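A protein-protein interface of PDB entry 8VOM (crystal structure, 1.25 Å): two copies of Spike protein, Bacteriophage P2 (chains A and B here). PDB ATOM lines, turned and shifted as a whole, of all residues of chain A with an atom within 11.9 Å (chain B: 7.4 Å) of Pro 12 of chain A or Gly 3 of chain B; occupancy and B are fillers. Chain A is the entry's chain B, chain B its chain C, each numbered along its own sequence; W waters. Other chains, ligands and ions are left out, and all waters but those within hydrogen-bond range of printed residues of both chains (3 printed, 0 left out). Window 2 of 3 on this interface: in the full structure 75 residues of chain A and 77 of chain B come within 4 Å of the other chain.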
ATOM      1  N   HIS A   8      -3.593   8.874   8.330  1.00  0.00           N
ATOM      2  CA  HIS A   8      -2.181   9.220   8.517  1.00  0.00           C
ATOM      3  C   HIS A   8      -2.135  10.710   8.196  1.00  0.00           C
ATOM      4  O   HIS A   8      -2.092  11.070   7.020  1.00  0.00           O
ATOM      5  CB  HIS A   8      -1.284   8.451   7.553  1.00  0.00           C
ATOM      6  CG  HIS A   8      -1.008   7.044   7.977  1.00  0.00           C
ATOM      7  ND1 HIS A   8      -1.567   5.953   7.349  1.00  0.00           N
ATOM      8  CD2 HIS A   8      -0.226   6.550   8.965  1.00  0.00           C
ATOM      9  CE1 HIS A   8      -1.154   4.849   7.946  1.00  0.00           C
ATOM     10  NE2 HIS A   8      -0.346   5.186   8.936  1.00  0.00           N
ATOM     11  N   ILE A   9      -2.201  11.561   9.211  1.00  0.00           N
ATOM     12  CA  ILE A   9      -2.098  13.004   9.031  1.00  0.00           C
ATOM     13  C   ILE A   9      -0.712  13.428   9.481  1.00  0.00           C
ATOM     14  O   ILE A   9      -0.340  13.203  10.638  1.00  0.00           O
ATOM     15  CB  ILE A   9      -3.167  13.768   9.828  1.00  0.00           C
ATOM     16  CG1 ILE A   9      -4.557  13.153   9.697  1.00  0.00           C
ATOM     17  CG2 ILE A   9      -3.148  15.222   9.413  1.00  0.00           C
ATOM     18  CD1 ILE A   9      -5.588  13.826  10.593  1.00  0.00           C
ATOM     19  N   ARG A  10       0.042  14.047   8.576  1.00  0.00           N
ATOM     20  CA  ARG A  10       1.426  14.445   8.815  1.00  0.00           C
ATOM     21  C   ARG A  10       1.495  15.955   8.672  1.00  0.00           C
ATOM     22  O   ARG A  10       1.403  16.486   7.563  1.00  0.00           O
ATOM     23  CB  ARG A  10       2.356  13.737   7.840  1.00  0.00           C
ATOM     24  CG  ARG A  10       2.218  12.209   7.896  1.00  0.00           C
ATOM     25  CD  ARG A  10       3.216  11.530   6.988  1.00  0.00           C
ATOM     26  NE  ARG A  10       2.859  10.157   6.637  1.00  0.00           N
ATOM     27  CZ  ARG A  10       3.035   9.080   7.390  1.00  0.00           C
ATOM     28  NH1 ARG A  10       3.682   9.135   8.547  1.00  0.00           N
ATOM     29  NH2 ARG A  10       2.570   7.908   6.958  1.00  0.00           N
ATOM     30  N   PHE A  11       1.644  16.623   9.780  1.00  0.00           N
ATOM     31  CA  PHE A  11       1.582  18.068   9.852  1.00  0.00           C
ATOM     32  C   PHE A  11       2.948  18.702   9.597  1.00  0.00           C
ATOM     33  O   PHE A  11       3.992  18.070   9.784  1.00  0.00           O
ATOM     34  CB  PHE A  11       1.095  18.463  11.234  1.00  0.00           C
ATOM     35  CG  PHE A  11      -0.298  17.999  11.550  1.00  0.00           C
ATOM     36  CD1 PHE A  11      -1.402  18.633  11.010  1.00  0.00           C
ATOM     37  CD2 PHE A  11      -0.507  16.930  12.404  1.00  0.00           C
ATOM     38  CE1 PHE A  11      -2.681  18.210  11.314  1.00  0.00           C
ATOM     39  CE2 PHE A  11      -1.791  16.520  12.726  1.00  0.00           C
ATOM     40  CZ  PHE A  11      -2.869  17.160  12.181  1.00  0.00           C
ATOM     41  N   PRO A  12       2.969  19.986   9.217  1.00  0.00           N
ATOM     42  CA  PRO A  12       4.239  20.628   8.839  1.00  0.00           C
ATOM     43  C   PRO A  12       5.193  20.884   9.986  1.00  0.00           C
ATOM     44  O   PRO A  12       6.353  21.225   9.714  1.00  0.00           O
ATOM     45  CB  PRO A  12       3.797  21.931   8.149  1.00  0.00           C
ATOM     46  CG  PRO A  12       2.420  22.182   8.618  1.00  0.00           C
ATOM     47  CD  PRO A  12       1.805  20.826   8.882  1.00  0.00           C
ATOM     48  N   ASP A  13       4.759  20.762  11.238  1.00  0.00           N
ATOM     49  CA  ASP A  13       5.641  20.884  12.390  1.00  0.00           C
ATOM     50  C   ASP A  13       6.219  19.544  12.831  1.00  0.00           C
ATOM     51  O   ASP A  13       6.881  19.484  13.872  1.00  0.00           O
ATOM     52  CB  ASP A  13       4.906  21.525  13.571  1.00  0.00           C
ATOM     53  CG  ASP A  13       3.758  20.667  14.077  1.00  0.00           C
ATOM     54  OD1 ASP A  13       3.339  19.728  13.347  1.00  0.00           O
ATOM     55  OD2 ASP A  13       3.323  20.914  15.222  1.00  0.00           O
ATOM     56  N   GLY A  14       5.966  18.471  12.081  1.00  0.00           N
ATOM     57  CA  GLY A  14       6.439  17.156  12.454  1.00  0.00           C
ATOM     58  C   GLY A  14       5.457  16.315  13.246  1.00  0.00           C
ATOM     59  O   GLY A  14       5.724  15.126  13.480  1.00  0.00           O
ATOM     60  N   ALA A  15       4.320  16.876  13.646  1.00  0.00           N
ATOM     61  CA  ALA A  15       3.321  16.082  14.348  1.00  0.00           C
ATOM     62  C   ALA A  15       2.648  15.087  13.406  1.00  0.00           C
ATOM     63  O   ALA A  15       2.537  15.311  12.197  1.00  0.00           O
ATOM     64  CB  ALA A  15       2.276  17.008  14.972  1.00  0.00           C
ATOM     65  N   VAL A  16       2.176  13.978  13.981  1.00  0.00           N
ATOM     66  CA  VAL A  16       1.476  12.949  13.224  1.00  0.00           C
ATOM     67  C   VAL A  16       0.302  12.442  14.048  1.00  0.00           C
ATOM     68  O   VAL A  16       0.415  12.246  15.261  1.00  0.00           O
ATOM     69  CB  VAL A  16       2.407  11.777  12.857  1.00  0.00           C
ATOM     70  CG1 VAL A  16       1.628  10.660  12.152  1.00  0.00           C
ATOM     71  CG2 VAL A  16       3.553  12.255  12.008  1.00  0.00           C
ATOM     72  N   ILE A  17      -0.830  12.247  13.380  1.00  0.00           N
ATOM     73  CA  ILE A  17      -1.970  11.522  13.931  1.00  0.00           C
ATOM     74  C   ILE A  17      -2.214  10.359  12.989  1.00  0.00           C
ATOM     75  O   ILE A  17      -2.412  10.565  11.788  1.00  0.00           O
ATOM     76  CB  ILE A  17      -3.217  12.414  14.021  1.00  0.00           C
ATOM     77  CG1 ILE A  17      -2.969  13.520  15.037  1.00  0.00           C
ATOM     78  CG2 ILE A  17      -4.455  11.602  14.412  1.00  0.00           C
ATOM     79  CD1 ILE A  17      -4.027  14.589  15.027  1.00  0.00           C
ATOM     80  N   SER A  29       1.590  12.000  17.966  1.00  0.00           N
ATOM     81  CA  SER A  29       2.967  12.267  18.342  1.00  0.00           C
ATOM     82  C   SER A  29       3.411  13.607  17.789  1.00  0.00           C
ATOM     83  O   SER A  29       2.835  14.134  16.837  1.00  0.00           O
ATOM     84  CB  SER A  29       3.889  11.172  17.822  1.00  0.00           C
ATOM     85  OG  SER A  29       3.900  11.198  16.414  1.00  0.00           O
ATOM     86  N   GLY A  30       4.487  14.129  18.377  1.00  0.00           N
ATOM     87  CA  GLY A  30       5.140  15.310  17.845  1.00  0.00           C
ATOM     88  C   GLY A  30       4.439  16.611  18.132  1.00  0.00           C
ATOM     89  O   GLY A  30       4.746  17.629  17.493  1.00  0.00           O
ATOM     90  N   ILE A  31       3.504  16.614  19.076  1.00  0.00           N
ATOM     91  CA  ILE A  31       2.753  17.798  19.441  1.00  0.00           C
ATOM     92  C   ILE A  31       3.364  18.414  20.690  1.00  0.00           C
ATOM     93  O   ILE A  31       4.111  17.777  21.426  1.00  0.00           O
ATOM     94  CB  ILE A  31       1.252  17.476  19.648  1.00  0.00           C
ATOM     95  CG1 ILE A  31       1.004  16.694  20.946  1.00  0.00           C
ATOM     96  CG2 ILE A  31       0.675  16.754  18.440  1.00  0.00           C
ATOM     97  CD1 ILE A  31      -0.461  16.411  21.241  1.00  0.00           C
ATOM     98  N   LYS A  32       3.012  19.675  20.949  1.00  0.00           N
ATOM     99  CA  LYS A  32       3.394  20.339  22.193  1.00  0.00           C
ATOM    100  C   LYS A  32       2.284  20.218  23.226  1.00  0.00           C
ATOM    101  O   LYS A  32       2.555  19.881  24.381  1.00  0.00           O
ATOM    102  CB  LYS A  32       3.725  21.813  21.926  1.00  0.00           C
ATOM    103  CG  LYS A  32       5.068  21.991  21.224  1.00  0.00           C
ATOM    104  CD  LYS A  32       5.425  23.465  21.007  1.00  0.00           C
ATOM    105  CE  LYS A  32       6.748  23.599  20.276  1.00  0.00           C
ATOM    106  NZ  LYS A  32       7.014  24.969  19.809  1.00  0.00           N
ATOM    107  N   GLY B   1       9.693  17.814   3.191  1.00  0.00           N
ATOM    108  CA  GLY B   1       9.416  18.523   4.430  1.00  0.00           C
ATOM    109  C   GLY B   1       8.795  17.608   5.468  1.00  0.00           C
ATOM    110  O   GLY B   1       8.651  16.415   5.203  1.00  0.00           O
ATOM    111  N   SER B   2       8.415  18.149   6.637  1.00  0.00           N
ATOM    112  CA  SER B   2       7.810  17.313   7.673  1.00  0.00           C
ATOM    113  C   SER B   2       6.409  16.826   7.311  1.00  0.00           C
ATOM    114  O   SER B   2       5.965  15.817   7.864  1.00  0.00           O
ATOM    115  CB  SER B   2       7.761  18.008   9.047  1.00  0.00           C
ATOM    116  OG  SER B   2       8.979  17.853   9.771  1.00  0.00           O
ATOM    117  N   GLY B   3       5.704  17.501   6.421  1.00  0.00           N
ATOM    118  CA  GLY B   3       4.331  17.149   6.103  1.00  0.00           C
ATOM    119  C   GLY B   3       3.543  18.384   5.728  1.00  0.00           C
ATOM    120  O   GLY B   3       3.882  19.508   6.086  1.00  0.00           O
ATOM    121  N   SER B   4       2.471  18.174   4.961  1.00  0.00           N
ATOM    122  CA  SER B   4       1.644  19.284   4.498  1.00  0.00           C
ATOM    123  C   SER B   4       0.177  19.144   4.887  1.00  0.00           C
ATOM    124  O   SER B   4      -0.649  19.942   4.424  1.00  0.00           O
ATOM    125  CB  SER B   4       1.730  19.442   2.976  1.00  0.00           C
ATOM    126  OG  SER B   4       1.418  18.221   2.328  1.00  0.00           O
ATOM    127  N   ASP B   5      -0.176  18.148   5.692  1.00  0.00           N
ATOM    128  CA  ASP B   5      -1.576  17.950   6.005  1.00  0.00           C
ATOM    129  C   ASP B   5      -2.056  18.952   7.032  1.00  0.00           C
ATOM    130  O   ASP B   5      -1.274  19.630   7.693  1.00  0.00           O
ATOM    131  CB  ASP B   5      -1.837  16.562   6.547  1.00  0.00           C
ATOM    132  CG  ASP B   5      -1.481  15.509   5.568  1.00  0.00           C
ATOM    133  OD1 ASP B   5      -1.599  15.761   4.352  1.00  0.00           O
ATOM    134  OD2 ASP B   5      -1.068  14.429   5.994  1.00  0.00           O
ATOM    135  N   ALA B   6      -3.378  19.004   7.179  1.00  0.00           N
ATOM    136  CA  ALA B   6      -4.029  19.952   8.060  1.00  0.00           C
ATOM    137  C   ALA B   6      -5.260  19.294   8.664  1.00  0.00           C
ATOM    138  O   ALA B   6      -5.789  18.309   8.139  1.00  0.00           O
ATOM    139  CB  ALA B   6      -4.435  21.222   7.306  1.00  0.00           C
ATOM    140  N   TYR B  19      -5.871  20.956  14.679  1.00  0.00           N
ATOM    141  CA  TYR B  19      -4.470  20.975  15.032  1.00  0.00           C
ATOM    142  C   TYR B  19      -3.902  22.279  14.504  1.00  0.00           C
ATOM    143  O   TYR B  19      -4.066  22.614  13.327  1.00  0.00           O
ATOM    144  CB  TYR B  19      -3.693  19.819  14.432  1.00  0.00           C
ATOM    145  CG  TYR B  19      -2.295  19.767  14.985  1.00  0.00           C
ATOM    146  CD1 TYR B  19      -2.089  19.458  16.315  1.00  0.00           C
ATOM    147  CD2 TYR B  19      -1.194  20.095  14.206  1.00  0.00           C
ATOM    148  CE1 TYR B  19      -0.828  19.436  16.849  1.00  0.00           C
ATOM    149  CE2 TYR B  19       0.082  20.069  14.731  1.00  0.00           C
ATOM    150  CZ  TYR B  19       0.256  19.726  16.058  1.00  0.00           C
ATOM    151  OH  TYR B  19       1.498  19.679  16.624  1.00  0.00           O
ATOM    152  N   PRO B  21      -0.524  23.924  13.813  1.00  0.00           N
ATOM    153  CA  PRO B  21       0.925  23.672  13.769  1.00  0.00           C
ATOM    154  C   PRO B  21       1.760  24.844  14.245  1.00  0.00           C
ATOM    155  O   PRO B  21       2.915  24.628  14.633  1.00  0.00           O
ATOM    156  CB  PRO B  21       1.200  23.380  12.294  1.00  0.00           C
ATOM    157  CG  PRO B  21      -0.008  23.898  11.576  1.00  0.00           C
ATOM    158  CD  PRO B  21      -1.153  23.909  12.487  1.00  0.00           C
ATOM    159  N   GLU B  22       1.207  26.071  14.250  1.00  0.00           N
ATOM    160  CA  GLU B  22       1.955  27.246  14.698  1.00  0.00           C
ATOM    161  C   GLU B  22       2.429  27.093  16.137  1.00  0.00           C
ATOM    162  O   GLU B  22       3.508  27.572  16.505  1.00  0.00           O
ATOM    163  CB  GLU B  22       1.084  28.514  14.612  1.00  0.00           C
ATOM    164  CG  GLU B  22       0.707  28.991  13.217  1.00  0.00           C
ATOM    165  CD  GLU B  22       1.902  29.542  12.510  1.00  0.00           C
ATOM    166  OE1 GLU B  22       2.498  28.783  11.716  1.00  0.00           O
ATOM    167  OE2 GLU B  22       2.282  30.693  12.793  1.00  0.00           O
HETATM  168  O   HOH W   1       5.169  24.830  17.533  1.00  0.00           O
HETATM  169  O   HOH W   2       1.634  15.528   4.325  1.00  0.00           O
HETATM  170  O   HOH W   3       7.742  21.084   7.357  1.00  0.00           O
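Among the printed residues, pairs that only touch across the chains: His 8 of chain A with Asp 5 of chain B, Ile 9 of chain A with Asp 5 of chain B, Arg 10 of chain A with Gly 3 of chain B, Phe 11 of chain A with Ser 2 of chain B, Phe 11 of chain A with Gly 3 of chain B, Phe 11 of chain A with Asp 5 of chain B, Phe 11 of chain A with Ala 6 of chain B, Phe 11 of chain A with Tyr 19 of chain B, Pro 12 of chain A with Ser 2 of chain B, Pro 12 of chain A with Asp 5 of chain B, Asp 13 of chain A with Pro 21 of chain B, Gly 14 of chain A with Ser 2 of chain B, Ala 15 of chain A with Tyr 19 of chain B, Gly 30 of chain A with Tyr 19 of chain B and Ile 31 of chain A with Tyr 19 of chain B.
N of Ile 9 of chain A sits at hydrogen-bond distance from O of Ile 17 of chain A (2.8 Å).
The side-chain carboxylate of Asp 13 of chain A is in hydrogen-bond range of the backbone NH of Ala 15 of chain A.
No position is printed for both chains.
Of the 19 pairs that touch across the chains among the printed residues, none has its exchanged pair printed and touching as well.
Pro 12 of chain A touches three residues of chain B.
No residue of chain A comes within 4 Å of Gly 1 of chain B.
Of chain A, only Phe 11, Pro 12 and Gly 14 come within 4 Å of Ser 2 of chain B.
Asp 5 of chain B touches just these residues of chain A: His 8, Ile 9, Arg 10, Phe 11 and Pro 12.
Printed residues of chain A within 4 Å of Pro 21 of chain B: Asp 13.
Of the printed residues of chain B, Ile 9 of chain A touches Asp 5 (3.4 Å).
Of the printed residues of chain A, Ala 6 of chain B touches Phe 11 (3.9 Å).
Printed residues of chain B within 4 Å of Gly 14 of chain A: Ser 2.
The nearest residue of chain B that does not touch Pro 12 of chain A is Pro 21 of chain B (4.1 Å).
The nearest residue of chain A that does not touch Gly 3 of chain B is Asp 13 of chain A (5.4 Å).
Water W3 bridges O of Pro 12 of chain A (2.7 Å) and N of Ser 2 of chain B (3.1 Å).
Water W2 lies within hydrogen-bond range of N of Ser 4 of chain B (2.8 Å), OD1 of Asp 5 of chain B (3.2 Å) and O of Arg 10 of chain A (3.4 Å).
Water W1 lies within hydrogen-bond range of the side-chain amino group (NZ) of Lys 32 of chain A (2.9 Å) and the backbone carbonyl oxygen (O) of Glu 22 of chain B (3.4 Å).
Of the 14 printed residues of chain A, 10 touch a printed residue of chain B.
Of the 9 printed residues of chain B, 7 touch a printed residue of chain A.
Among the printed residues, 19 pairs touch across the chains.
Among the printed residues, no Asp or Glu carboxylate lies within 4 Å of a Lys or Arg side-chain nitrogen of the other chain.
N of Ser 4 of chain B sits at hydrogen-bond distance from O of Arg 10 of chain A, at 3.3 Å.
The backbone NH of Arg 10 of chain A lies within hydrogen-bond range of the side-chain carboxylate of Asp 5 of chain B (2.8 Å).
OD2 of Asp 13 of chain A sits at hydrogen-bond distance from OH of Tyr 19 of chain B (2.6 Å).
The backbone carbonyl oxygen of Gly 3 of chain B lies close to the backbone nitrogen of Pro 12 of chain A (3.3 Å).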
